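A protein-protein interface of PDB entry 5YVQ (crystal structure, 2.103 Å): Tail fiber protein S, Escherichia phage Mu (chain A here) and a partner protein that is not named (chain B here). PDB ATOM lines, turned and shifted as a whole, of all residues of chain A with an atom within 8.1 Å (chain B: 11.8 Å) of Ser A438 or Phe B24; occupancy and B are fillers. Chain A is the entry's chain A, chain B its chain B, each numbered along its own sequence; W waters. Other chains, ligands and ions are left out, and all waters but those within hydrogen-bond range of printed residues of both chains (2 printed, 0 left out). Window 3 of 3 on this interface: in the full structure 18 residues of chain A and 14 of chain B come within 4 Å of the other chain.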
ATOM      1  N   TYR A 433      16.121  -9.203  -6.488  1.00  0.00           N
ATOM      2  CA  TYR A 433      16.820  -8.176  -7.252  1.00  0.00           C
ATOM      3  C   TYR A 433      16.608  -6.770  -6.706  1.00  0.00           C
ATOM      4  O   TYR A 433      16.999  -5.804  -7.370  1.00  0.00           O
ATOM      5  CB  TYR A 433      16.375  -8.206  -8.713  1.00  0.00           C
ATOM      6  CG  TYR A 433      16.898  -9.358  -9.562  1.00  0.00           C
ATOM      7  CD1 TYR A 433      16.184 -10.550  -9.665  1.00  0.00           C
ATOM      8  CD2 TYR A 433      18.074  -9.234 -10.294  1.00  0.00           C
ATOM      9  CE1 TYR A 433      16.641 -11.600 -10.460  1.00  0.00           C
ATOM     10  CE2 TYR A 433      18.545 -10.289 -11.102  1.00  0.00           C
ATOM     11  CZ  TYR A 433      17.819 -11.459 -11.181  1.00  0.00           C
ATOM     12  OH  TYR A 433      18.262 -12.497 -11.980  1.00  0.00           O
ATOM     13  N   ALA A 434      16.011  -6.637  -5.513  1.00  0.00           N
ATOM     14  CA  ALA A 434      15.549  -5.337  -5.034  1.00  0.00           C
ATOM     15  C   ALA A 434      16.655  -4.282  -5.027  1.00  0.00           C
ATOM     16  O   ALA A 434      16.411  -3.119  -5.370  1.00  0.00           O
ATOM     17  CB  ALA A 434      14.946  -5.478  -3.637  1.00  0.00           C
ATOM     18  N   ASN A 435      17.876  -4.656  -4.644  1.00  0.00           N
ATOM     19  CA  ASN A 435      18.937  -3.655  -4.575  1.00  0.00           C
ATOM     20  C   ASN A 435      19.430  -3.221  -5.948  1.00  0.00           C
ATOM     21  O   ASN A 435      20.108  -2.189  -6.036  1.00  0.00           O
ATOM     22  CB  ASN A 435      20.127  -4.172  -3.762  1.00  0.00           C
ATOM     23  CG  ASN A 435      20.657  -5.482  -4.288  1.00  0.00           C
ATOM     24  OD1 ASN A 435      19.907  -6.449  -4.421  1.00  0.00           O
ATOM     25  ND2 ASN A 435      21.955  -5.522  -4.602  1.00  0.00           N
ATOM     26  N   PHE A 436      19.142  -3.996  -7.003  1.00  0.00           N
ATOM     27  CA  PHE A 436      19.368  -3.571  -8.384  1.00  0.00           C
ATOM     28  C   PHE A 436      18.145  -2.835  -8.967  1.00  0.00           C
ATOM     29  O   PHE A 436      18.284  -1.771  -9.585  1.00  0.00           O
ATOM     30  CB  PHE A 436      19.721  -4.789  -9.258  1.00  0.00           C
ATOM     31  CG  PHE A 436      21.058  -5.420  -8.936  1.00  0.00           C
ATOM     32  CD1 PHE A 436      22.223  -4.920  -9.493  1.00  0.00           C
ATOM     33  CD2 PHE A 436      21.139  -6.510  -8.079  1.00  0.00           C
ATOM     34  CE1 PHE A 436      23.458  -5.488  -9.198  1.00  0.00           C
ATOM     35  CE2 PHE A 436      22.391  -7.096  -7.775  1.00  0.00           C
ATOM     36  CZ  PHE A 436      23.543  -6.579  -8.342  1.00  0.00           C
ATOM     37  N   ASP A 437      16.938  -3.390  -8.776  1.00  0.00           N
ATOM     38  CA  ASP A 437      15.735  -2.798  -9.359  1.00  0.00           C
ATOM     39  C   ASP A 437      15.489  -1.382  -8.869  1.00  0.00           C
ATOM     40  O   ASP A 437      14.802  -0.612  -9.549  1.00  0.00           O
ATOM     41  CB  ASP A 437      14.515  -3.665  -9.053  1.00  0.00           C
ATOM     42  CG  ASP A 437      14.515  -4.964  -9.843  1.00  0.00           C
ATOM     43  OD1 ASP A 437      15.417  -5.151 -10.696  1.00  0.00           O
ATOM     44  OD2 ASP A 437      13.628  -5.805  -9.589  1.00  0.00           O
ATOM     45  N   SER A 438      16.034  -1.017  -7.718  1.00  0.00           N
ATOM     46  CA  SER A 438      15.882   0.336  -7.206  1.00  0.00           C
ATOM     47  C   SER A 438      16.885   1.321  -7.793  1.00  0.00           C
ATOM     48  O   SER A 438      16.876   2.490  -7.398  1.00  0.00           O
ATOM     49  CB  SER A 438      16.030   0.329  -5.690  1.00  0.00           C
ATOM     50  OG  SER A 438      17.388   0.080  -5.398  1.00  0.00           O
ATOM     51  N   ARG A 439      17.753   0.896  -8.707  1.00  0.00           N
ATOM     52  CA  ARG A 439      18.753   1.804  -9.252  1.00  0.00           C
ATOM     53  C   ARG A 439      18.438   2.318 -10.652  1.00  0.00           C
ATOM     54  O   ARG A 439      19.040   3.312 -11.060  1.00  0.00           O
ATOM     55  CB  ARG A 439      20.122   1.135  -9.299  1.00  0.00           C
ATOM     56  CG  ARG A 439      20.614   0.640  -7.956  1.00  0.00           C
ATOM     57  CD  ARG A 439      21.982  -0.011  -8.085  1.00  0.00           C
ATOM     58  NE  ARG A 439      23.077   0.934  -8.306  1.00  0.00           N
ATOM     59  CZ  ARG A 439      23.686   1.631  -7.342  1.00  0.00           C
ATOM     60  NH1 ARG A 439      23.273   1.525  -6.077  1.00  0.00           N
ATOM     61  NH2 ARG A 439      24.697   2.449  -7.646  1.00  0.00           N
ATOM     62  N   TYR A 440      17.535   1.678 -11.402  1.00  0.00           N
ATOM     63  CA  TYR A 440      17.478   1.891 -12.843  1.00  0.00           C
ATOM     64  C   TYR A 440      16.045   2.095 -13.328  1.00  0.00           C
ATOM     65  O   TYR A 440      15.076   1.718 -12.666  1.00  0.00           O
ATOM     66  CB  TYR A 440      18.133   0.718 -13.610  1.00  0.00           C
ATOM     67  CG  TYR A 440      19.502   0.321 -13.070  1.00  0.00           C
ATOM     68  CD1 TYR A 440      20.562   1.223 -13.083  1.00  0.00           C
ATOM     69  CD2 TYR A 440      19.732  -0.950 -12.550  1.00  0.00           C
ATOM     70  CE1 TYR A 440      21.806   0.878 -12.582  1.00  0.00           C
ATOM     71  CE2 TYR A 440      20.985  -1.304 -12.050  1.00  0.00           C
ATOM     72  CZ  TYR A 440      22.017  -0.380 -12.075  1.00  0.00           C
ATOM     73  OH  TYR A 440      23.273  -0.695 -11.591  1.00  0.00           O
ATOM     74  N   VAL A 441      15.932   2.715 -14.499  1.00  0.00           N
ATOM     75  CA  VAL A 441      14.664   2.796 -15.214  1.00  0.00           C
ATOM     76  C   VAL A 441      14.398   1.448 -15.861  1.00  0.00           C
ATOM     77  O   VAL A 441      15.241   0.929 -16.602  1.00  0.00           O
ATOM     78  CB  VAL A 441      14.698   3.914 -16.274  1.00  0.00           C
ATOM     79  CG1 VAL A 441      13.410   3.918 -17.086  1.00  0.00           C
ATOM     80  CG2 VAL A 441      14.913   5.267 -15.623  1.00  0.00           C
ATOM     81  N   LYS A 492       8.161   7.293 -16.476  1.00  0.00           N
ATOM     82  CA  LYS A 492       9.251   6.350 -16.259  1.00  0.00           C
ATOM     83  C   LYS A 492       8.867   5.360 -15.170  1.00  0.00           C
ATOM     84  O   LYS A 492       8.257   5.729 -14.160  1.00  0.00           O
ATOM     85  CB  LYS A 492      10.555   7.059 -15.860  1.00  0.00           C
ATOM     86  CG  LYS A 492      10.443   7.872 -14.588  1.00  0.00           C
ATOM     87  CD  LYS A 492      11.654   8.751 -14.372  1.00  0.00           C
ATOM     88  CE  LYS A 492      11.437   9.686 -13.199  1.00  0.00           C
ATOM     89  NZ  LYS A 492      12.571  10.639 -13.056  1.00  0.00           N
ATOM     90  N   ASN A 493       9.215   4.106 -15.379  1.00  0.00           N
ATOM     91  CA  ASN A 493       8.921   3.059 -14.412  1.00  0.00           C
ATOM     92  C   ASN A 493      10.201   2.753 -13.636  1.00  0.00           C
ATOM     93  O   ASN A 493      11.152   2.197 -14.190  1.00  0.00           O
ATOM     94  CB  ASN A 493       8.373   1.819 -15.111  1.00  0.00           C
ATOM     95  CG  ASN A 493       7.905   0.761 -14.134  1.00  0.00           C
ATOM     96  OD1 ASN A 493       8.562   0.492 -13.136  1.00  0.00           O
ATOM     97  ND2 ASN A 493       6.768   0.157 -14.416  1.00  0.00           N
ATOM     98  N   ILE A 494      10.218   3.114 -12.355  1.00  0.00           N
ATOM     99  CA  ILE A 494      11.309   2.773 -11.441  1.00  0.00           C
ATOM    100  C   ILE A 494      10.800   1.723 -10.468  1.00  0.00           C
ATOM    101  O   ILE A 494       9.905   1.998  -9.657  1.00  0.00           O
ATOM    102  CB  ILE A 494      11.819   4.001 -10.666  1.00  0.00           C
ATOM    103  CG1 ILE A 494      11.957   5.224 -11.583  1.00  0.00           C
ATOM    104  CG2 ILE A 494      13.117   3.660  -9.919  1.00  0.00           C
ATOM    105  CD1 ILE A 494      12.998   5.064 -12.650  1.00  0.00           C
ATOM    106  N   ASN A 495      11.376   0.525 -10.524  1.00  0.00           N
ATOM    107  CA  ASN A 495      11.143  -0.456  -9.470  1.00  0.00           C
ATOM    108  C   ASN A 495       9.668  -0.834  -9.370  1.00  0.00           C
ATOM    109  O   ASN A 495       9.166  -1.144  -8.286  1.00  0.00           O
ATOM    110  CB  ASN A 495      11.654   0.080  -8.129  1.00  0.00           C
ATOM    111  CG  ASN A 495      11.862  -1.008  -7.094  1.00  0.00           C
ATOM    112  OD1 ASN A 495      12.018  -2.188  -7.420  1.00  0.00           O
ATOM    113  ND2 ASN A 495      11.859  -0.609  -5.831  1.00  0.00           N
ATOM    114  N   GLY A 496       8.949  -0.773 -10.490  1.00  0.00           N
ATOM    115  CA  GLY A 496       7.581  -1.228 -10.532  1.00  0.00           C
ATOM    116  C   GLY A 496       6.528  -0.154 -10.377  1.00  0.00           C
ATOM    117  O   GLY A 496       5.340  -0.469 -10.457  1.00  0.00           O
ATOM    118  N   TYR A 499       6.217   6.755 -12.597  1.00  0.00           N
ATOM    119  CA  TYR A 499       6.303   8.123 -12.115  1.00  0.00           C
ATOM    120  C   TYR A 499       6.290   9.075 -13.303  1.00  0.00           C
ATOM    121  O   TYR A 499       6.750   8.742 -14.401  1.00  0.00           O
ATOM    122  CB  TYR A 499       7.571   8.366 -11.278  1.00  0.00           C
ATOM    123  CG  TYR A 499       7.674   7.550 -10.002  1.00  0.00           C
ATOM    124  CD1 TYR A 499       6.996   7.925  -8.847  1.00  0.00           C
ATOM    125  CD2 TYR A 499       8.470   6.409  -9.952  1.00  0.00           C
ATOM    126  CE1 TYR A 499       7.095   7.173  -7.679  1.00  0.00           C
ATOM    127  CE2 TYR A 499       8.586   5.657  -8.795  1.00  0.00           C
ATOM    128  CZ  TYR A 499       7.896   6.039  -7.660  1.00  0.00           C
ATOM    129  OH  TYR A 499       8.010   5.281  -6.510  1.00  0.00           O
ATOM    130  N   ASN A 500       5.772  10.273 -13.081  1.00  0.00           N
ATOM    131  CA  ASN A 500       5.786  11.266 -14.138  1.00  0.00           C
ATOM    132  C   ASN A 500       7.149  11.941 -14.212  1.00  0.00           C
ATOM    133  O   ASN A 500       7.767  12.265 -13.192  1.00  0.00           O
ATOM    134  CB  ASN A 500       4.670  12.283 -13.921  1.00  0.00           C
ATOM    135  CG  ASN A 500       3.303  11.672 -14.141  1.00  0.00           C
ATOM    136  OD1 ASN A 500       2.923  11.385 -15.273  1.00  0.00           O
ATOM    137  ND2 ASN A 500       2.571  11.437 -13.055  1.00  0.00           N
ATOM    138  N   VAL A 501       7.629  12.116 -15.439  1.00  0.00           N
ATOM    139  CA  VAL A 501       8.899  12.780 -15.674  1.00  0.00           C
ATOM    140  C   VAL A 501       8.788  14.255 -15.294  1.00  0.00           C
ATOM    141  O   VAL A 501       7.705  14.847 -15.331  1.00  0.00           O
ATOM    142  CB  VAL A 501       9.290  12.574 -17.150  1.00  0.00           C
ATOM    143  CG1 VAL A 501      10.182  13.687 -17.680  1.00  0.00           C
ATOM    144  CG2 VAL A 501       9.942  11.201 -17.308  1.00  0.00           C
ATOM    145  N   ALA A 502       9.903  14.840 -14.869  1.00  0.00           N
ATOM    146  CA  ALA A 502       9.949  16.251 -14.526  1.00  0.00           C
ATOM    147  C   ALA A 502      10.495  17.062 -15.694  1.00  0.00           C
ATOM    148  O   ALA A 502      11.313  16.578 -16.484  1.00  0.00           O
ATOM    149  CB  ALA A 502      10.816  16.498 -13.291  1.00  0.00           C
ATOM    150  N   PRO B  12       8.440  16.010  -0.561  1.00  0.00           N
ATOM    151  CA  PRO B  12       8.334  14.683   0.058  1.00  0.00           C
ATOM    152  C   PRO B  12       8.263  14.805   1.572  1.00  0.00           C
ATOM    153  O   PRO B  12       8.918  15.656   2.177  1.00  0.00           O
ATOM    154  CB  PRO B  12       9.613  13.971  -0.399  1.00  0.00           C
ATOM    155  CG  PRO B  12      10.563  15.069  -0.733  1.00  0.00           C
ATOM    156  CD  PRO B  12       9.714  16.180  -1.283  1.00  0.00           C
ATOM    157  N   LYS B  15      11.089   9.592   4.527  1.00  0.00           N
ATOM    158  CA  LYS B  15      12.450   9.290   4.097  1.00  0.00           C
ATOM    159  C   LYS B  15      12.466   8.607   2.732  1.00  0.00           C
ATOM    160  O   LYS B  15      13.303   8.935   1.882  1.00  0.00           O
ATOM    161  CB  LYS B  15      13.157   8.431   5.155  1.00  0.00           C
ATOM    162  CG  LYS B  15      12.653   6.993   5.268  1.00  0.00           C
ATOM    163  CD  LYS B  15      13.404   6.192   6.329  1.00  0.00           C
ATOM    164  CE  LYS B  15      13.741   4.795   5.821  1.00  0.00           C
ATOM    165  NZ  LYS B  15      12.692   4.258   4.904  1.00  0.00           N
ATOM    166  N   GLU B  16      11.546   7.667   2.498  1.00  0.00           N
ATOM    167  CA  GLU B  16      11.538   6.947   1.229  1.00  0.00           C
ATOM    168  C   GLU B  16      11.131   7.871   0.089  1.00  0.00           C
ATOM    169  O   GLU B  16      11.702   7.810  -1.006  1.00  0.00           O
ATOM    170  CB  GLU B  16      10.607   5.739   1.319  1.00  0.00           C
ATOM    171  CG  GLU B  16      10.685   4.790   0.135  1.00  0.00           C
ATOM    172  CD  GLU B  16      10.188   3.389   0.471  1.00  0.00           C
ATOM    173  OE1 GLU B  16       9.486   3.229   1.495  1.00  0.00           O
ATOM    174  OE2 GLU B  16      10.511   2.445  -0.285  1.00  0.00           O
ATOM    175  N   GLN B  17      10.158   8.746   0.335  1.00  0.00           N
ATOM    176  CA  GLN B  17       9.830   9.770  -0.646  1.00  0.00           C
ATOM    177  C   GLN B  17      10.993  10.732  -0.852  1.00  0.00           C
ATOM    178  O   GLN B  17      11.225  11.198  -1.978  1.00  0.00           O
ATOM    179  CB  GLN B  17       8.569  10.514  -0.208  1.00  0.00           C
ATOM    180  CG  GLN B  17       7.322   9.648  -0.250  1.00  0.00           C
ATOM    181  CD  GLN B  17       6.371   9.909   0.902  1.00  0.00           C
ATOM    182  OE1 GLN B  17       5.881   8.974   1.539  1.00  0.00           O
ATOM    183  NE2 GLN B  17       6.097  11.183   1.169  1.00  0.00           N
ATOM    184  N   TYR B  18      11.754  11.015   0.211  1.00  0.00           N
ATOM    185  CA  TYR B  18      12.891  11.922   0.086  1.00  0.00           C
ATOM    186  C   TYR B  18      14.002  11.310  -0.758  1.00  0.00           C
ATOM    187  O   TYR B  18      14.691  12.022  -1.498  1.00  0.00           O
ATOM    188  CB  TYR B  18      13.421  12.302   1.467  1.00  0.00           C
ATOM    189  CG  TYR B  18      14.616  13.226   1.406  1.00  0.00           C
ATOM    190  CD1 TYR B  18      14.451  14.592   1.221  1.00  0.00           C
ATOM    191  CD2 TYR B  18      15.909  12.732   1.515  1.00  0.00           C
ATOM    192  CE1 TYR B  18      15.540  15.440   1.156  1.00  0.00           C
ATOM    193  CE2 TYR B  18      17.001  13.571   1.449  1.00  0.00           C
ATOM    194  CZ  TYR B  18      16.813  14.921   1.271  1.00  0.00           C
ATOM    195  OH  TYR B  18      17.899  15.762   1.208  1.00  0.00           O
ATOM    196  N   GLN B  19      14.206   9.998  -0.653  1.00  0.00           N
ATOM    197  CA  GLN B  19      15.240   9.362  -1.460  1.00  0.00           C
ATOM    198  C   GLN B  19      14.860   9.368  -2.934  1.00  0.00           C
ATOM    199  O   GLN B  19      15.700   9.648  -3.797  1.00  0.00           O
ATOM    200  CB  GLN B  19      15.484   7.932  -0.979  1.00  0.00           C
ATOM    201  CG  GLN B  19      16.245   7.845   0.329  1.00  0.00           C
ATOM    202  CD  GLN B  19      17.596   8.527   0.267  1.00  0.00           C
ATOM    203  OE1 GLN B  19      17.885   9.423   1.060  1.00  0.00           O
ATOM    204  NE2 GLN B  19      18.436   8.100  -0.669  1.00  0.00           N
ATOM    205  N   LEU B  20      13.601   9.052  -3.234  1.00  0.00           N
ATOM    206  CA  LEU B  20      13.152   9.006  -4.619  1.00  0.00           C
ATOM    207  C   LEU B  20      13.191  10.387  -5.264  1.00  0.00           C
ATOM    208  O   LEU B  20      13.514  10.513  -6.453  1.00  0.00           O
ATOM    209  CB  LEU B  20      11.747   8.410  -4.683  1.00  0.00           C
ATOM    210  CG  LEU B  20      11.697   6.885  -4.547  1.00  0.00           C
ATOM    211  CD1 LEU B  20      10.319   6.431  -4.081  1.00  0.00           C
ATOM    212  CD2 LEU B  20      12.066   6.229  -5.878  1.00  0.00           C
ATOM    213  N   THR B  21      12.863  11.436  -4.505  1.00  0.00           N
ATOM    214  CA  THR B  21      13.014  12.781  -5.049  1.00  0.00           C
ATOM    215  C   THR B  21      14.487  13.167  -5.166  1.00  0.00           C
ATOM    216  O   THR B  21      14.875  13.858  -6.114  1.00  0.00           O
ATOM    217  CB  THR B  21      12.236  13.794  -4.194  1.00  0.00           C
ATOM    218  OG1 THR B  21      10.825  13.584  -4.354  1.00  0.00           O
ATOM    219  CG2 THR B  21      12.555  15.224  -4.606  1.00  0.00           C
ATOM    220  N   LYS B  22      15.330  12.701  -4.243  1.00  0.00           N
ATOM    221  CA  LYS B  22      16.743  13.060  -4.295  1.00  0.00           C
ATOM    222  C   LYS B  22      17.446  12.377  -5.465  1.00  0.00           C
ATOM    223  O   LYS B  22      18.294  12.986  -6.125  1.00  0.00           O
ATOM    224  CB  LYS B  22      17.417  12.704  -2.965  1.00  0.00           C
ATOM    225  CG  LYS B  22      18.939  12.816  -2.954  1.00  0.00           C
ATOM    226  CD  LYS B  22      19.472  12.920  -1.532  1.00  0.00           C
ATOM    227  CE  LYS B  22      20.976  12.668  -1.471  1.00  0.00           C
ATOM    228  NZ  LYS B  22      21.322  11.225  -1.620  1.00  0.00           N
ATOM    229  N   ASN B  23      17.101  11.120  -5.743  1.00  0.00           N
ATOM    230  CA  ASN B  23      17.791  10.326  -6.755  1.00  0.00           C
ATOM    231  C   ASN B  23      17.103  10.326  -8.119  1.00  0.00           C
ATOM    232  O   ASN B  23      17.789  10.211  -9.141  1.00  0.00           O
ATOM    233  CB  ASN B  23      17.943   8.874  -6.282  1.00  0.00           C
ATOM    234  CG  ASN B  23      18.870   8.733  -5.072  1.00  0.00           C
ATOM    235  OD1 ASN B  23      19.721   9.587  -4.812  1.00  0.00           O
ATOM    236  ND2 ASN B  23      18.705   7.643  -4.333  1.00  0.00           N
ATOM    237  N   PHE B  24      15.772  10.435  -8.169  1.00  0.00           N
ATOM    238  CA  PHE B  24      15.043  10.330  -9.429  1.00  0.00           C
ATOM    239  C   PHE B  24      14.120  11.522  -9.682  1.00  0.00           C
ATOM    240  O   PHE B  24      13.290  11.465 -10.599  1.00  0.00           O
ATOM    241  CB  PHE B  24      14.246   9.019  -9.478  1.00  0.00           C
ATOM    242  CG  PHE B  24      15.092   7.776  -9.280  1.00  0.00           C
ATOM    243  CD1 PHE B  24      15.730   7.167 -10.357  1.00  0.00           C
ATOM    244  CD2 PHE B  24      15.249   7.219  -8.015  1.00  0.00           C
ATOM    245  CE1 PHE B  24      16.513   6.019 -10.176  1.00  0.00           C
ATOM    246  CE2 PHE B  24      16.025   6.071  -7.819  1.00  0.00           C
ATOM    247  CZ  PHE B  24      16.661   5.471  -8.897  1.00  0.00           C
ATOM    248  N   ASP B  25      14.248  12.598  -8.898  1.00  0.00           N
ATOM    249  CA  ASP B  25      13.507  13.848  -9.104  1.00  0.00           C
ATOM    250  C   ASP B  25      11.997  13.638  -9.073  1.00  0.00           C
ATOM    251  O   ASP B  25      11.253  14.365  -9.741  1.00  0.00           O
ATOM    252  CB  ASP B  25      13.900  14.531 -10.417  1.00  0.00           C
ATOM    253  CG  ASP B  25      15.327  15.018 -10.417  1.00  0.00           C
ATOM    254  OD1 ASP B  25      15.887  15.208  -9.315  1.00  0.00           O
ATOM    255  OD2 ASP B  25      15.881  15.224 -11.521  1.00  0.00           O
ATOM    256  N   VAL B  26      11.537  12.636  -8.315  1.00  0.00           N
ATOM    257  CA  VAL B  26      10.109  12.366  -8.230  1.00  0.00           C
ATOM    258  C   VAL B  26       9.399  13.590  -7.668  1.00  0.00           C
ATOM    259  O   VAL B  26       9.781  14.125  -6.619  1.00  0.00           O
ATOM    260  CB  VAL B  26       9.851  11.114  -7.378  1.00  0.00           C
ATOM    261  CG1 VAL B  26       8.393  11.022  -6.999  1.00  0.00           C
ATOM    262  CG2 VAL B  26      10.270   9.858  -8.136  1.00  0.00           C
ATOM    263  N   ILE B  27       8.377  14.055  -8.378  1.00  0.00           N
ATOM    264  CA  ILE B  27       7.539  15.154  -7.927  1.00  0.00           C
ATOM    265  C   ILE B  27       6.310  14.531  -7.278  1.00  0.00           C
ATOM    266  O   ILE B  27       5.428  14.011  -7.968  1.00  0.00           O
ATOM    267  CB  ILE B  27       7.164  16.092  -9.088  1.00  0.00           C
ATOM    268  CG1 ILE B  27       8.422  16.755  -9.658  1.00  0.00           C
ATOM    269  CG2 ILE B  27       6.159  17.147  -8.639  1.00  0.00           C
ATOM    270  CD1 ILE B  27       8.163  17.638 -10.859  1.00  0.00           C
ATOM    271  N   TRP B  28       6.252  14.560  -5.950  1.00  0.00           N
ATOM    272  CA  TRP B  28       5.170  13.906  -5.223  1.00  0.00           C
ATOM    273  C   TRP B  28       3.894  14.738  -5.291  1.00  0.00           C
ATOM    274  O   TRP B  28       3.898  15.933  -4.981  1.00  0.00           O
ATOM    275  CB  TRP B  28       5.579  13.657  -3.771  1.00  0.00           C
ATOM    276  CG  TRP B  28       6.692  12.681  -3.674  1.00  0.00           C
ATOM    277  CD1 TRP B  28       8.021  12.958  -3.547  1.00  0.00           C
ATOM    278  CD2 TRP B  28       6.582  11.258  -3.733  1.00  0.00           C
ATOM    279  NE1 TRP B  28       8.750  11.790  -3.513  1.00  0.00           N
ATOM    280  CE2 TRP B  28       7.886  10.732  -3.619  1.00  0.00           C
ATOM    281  CE3 TRP B  28       5.506  10.376  -3.858  1.00  0.00           C
ATOM    282  CZ2 TRP B  28       8.140   9.369  -3.640  1.00  0.00           C
ATOM    283  CZ3 TRP B  28       5.764   9.020  -3.866  1.00  0.00           C
ATOM    284  CH2 TRP B  28       7.070   8.531  -3.761  1.00  0.00           C
ATOM    285  N   TYR B  38       0.533   8.783  -5.898  1.00  0.00           N
ATOM    286  CA  TYR B  38       1.235   7.613  -6.427  1.00  0.00           C
ATOM    287  C   TYR B  38       0.953   6.353  -5.619  1.00  0.00           C
ATOM    288  O   TYR B  38       0.984   5.249  -6.174  1.00  0.00           O
ATOM    289  CB  TYR B  38       2.745   7.870  -6.495  1.00  0.00           C
ATOM    290  CG  TYR B  38       3.129   8.736  -7.671  1.00  0.00           C
ATOM    291  CD1 TYR B  38       2.856   8.336  -8.971  1.00  0.00           C
ATOM    292  CD2 TYR B  38       3.727   9.979  -7.479  1.00  0.00           C
ATOM    293  CE1 TYR B  38       3.189   9.136 -10.048  1.00  0.00           C
ATOM    294  CE2 TYR B  38       4.063  10.784  -8.549  1.00  0.00           C
ATOM    295  CZ  TYR B  38       3.796  10.356  -9.828  1.00  0.00           C
ATOM    296  OH  TYR B  38       4.121  11.163 -10.892  1.00  0.00           O
HETATM  297  O   HOH W   1      10.198  12.664 -11.927  1.00  0.00           O
HETATM  298  O   HOH W   2       7.196  12.443 -10.526  1.00  0.00           O
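No residue of chain B comes within 4 Å of Ala A434.
No residue of chain B comes within 4 Å of Asn A435.
Ser A438 touches just one residue of chain B: Phe B24 (3.3 Å).
No residue of chain B comes within 4 Å of Tyr A440.
Of the printed residues of chain B, Lys A492 touches Phe B24 (2.7 Å).
No residue of chain B comes within 4 Å of Ile A494.
Of the printed residues of chain B, Tyr A499 touches Leu B20, Val B26 and Tyr B38.
Of the printed residues of chain B, Asn A500 touches Tyr B38 (2.7 Å).
Of the printed residues of chain B, Ala A502 touches Ile B27 (3.8 Å).
Of chain A, only Ser A438, Arg A439 and Lys A492 come within 4 Å of Phe B24.
Of the printed residues of chain A, Tyr B38 touches Tyr A499 and Asn A500.
The nearest residue of chain A that does not touch Phe B24 is Ile A494 (4.1 Å).
The nearest printed residue of chain A that does not touch Tyr B38 is Val A501 (5.8 Å).
Among the printed residues, merely in contact across the chains: Ser A438 with Phe B24 (3.3 Å), Arg A439 with Phe B24 (3.8 Å), Tyr A499 with Leu B20 (3.5 Å), Tyr A499 with Val B26 (3.9 Å), Tyr A499 with Tyr B38 (3.9 Å) and Ala A502 with Ile B27 (3.8 Å).
NZ of Lys A492 is in hydrogen-bond range of O of Phe B24, 2.7 Å away.
The side-chain amide nitrogen (ND2) of Asn A500 is in hydrogen-bond range of the side-chain hydroxyl (OH) of Tyr B38, 2.7 Å away.
Water W2 lies within hydrogen-bond range of the backbone carbonyl oxygen of Asn A500, the backbone NH of Ile B27 and the side-chain hydroxyl of Tyr B38.
Water W1 lies within hydrogen-bond range of O of Asn A500 (2.8 Å), O of Asp B25 (3.0 Å) and NZ of Lys A492 (3.3 Å).
Hydrophobic or aromatic side chains of chain A within 4 Å of the printed part of chain B: Tyr A499 and Ala A502.
Hydrophobic or aromatic side chains of chain B that line the printed part of chain A: Leu B20, Phe B24, Val B26, Ile B27 and Tyr B38.
Among the printed residues, 8 pairs touch across the chains.
Among the printed residues, no Asp or Glu carboxylate lies within 4 Å of a Lys or Arg side-chain nitrogen of the other chain.
O of Lys A492 lies within hydrogen-bond range of N of Tyr A499 (2.8 Å).
The backbone carbonyl oxygen (O) of Ala A434 sits at hydrogen-bond distance from the side-chain hydroxyl (OG) of Ser A438, 3.3 Å away.
O of Val B26 lies within hydrogen-bond range of OG1 of Thr B21, at 2.6 Å.
The backbone carbonyl oxygen (O) of Leu B20 lies within hydrogen-bond range of the backbone NH (N) of Val B26 (3.4 Å).
The backbone NH (N) of Asp B25 lies within hydrogen-bond range of the backbone carbonyl oxygen (O) of Leu B20.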
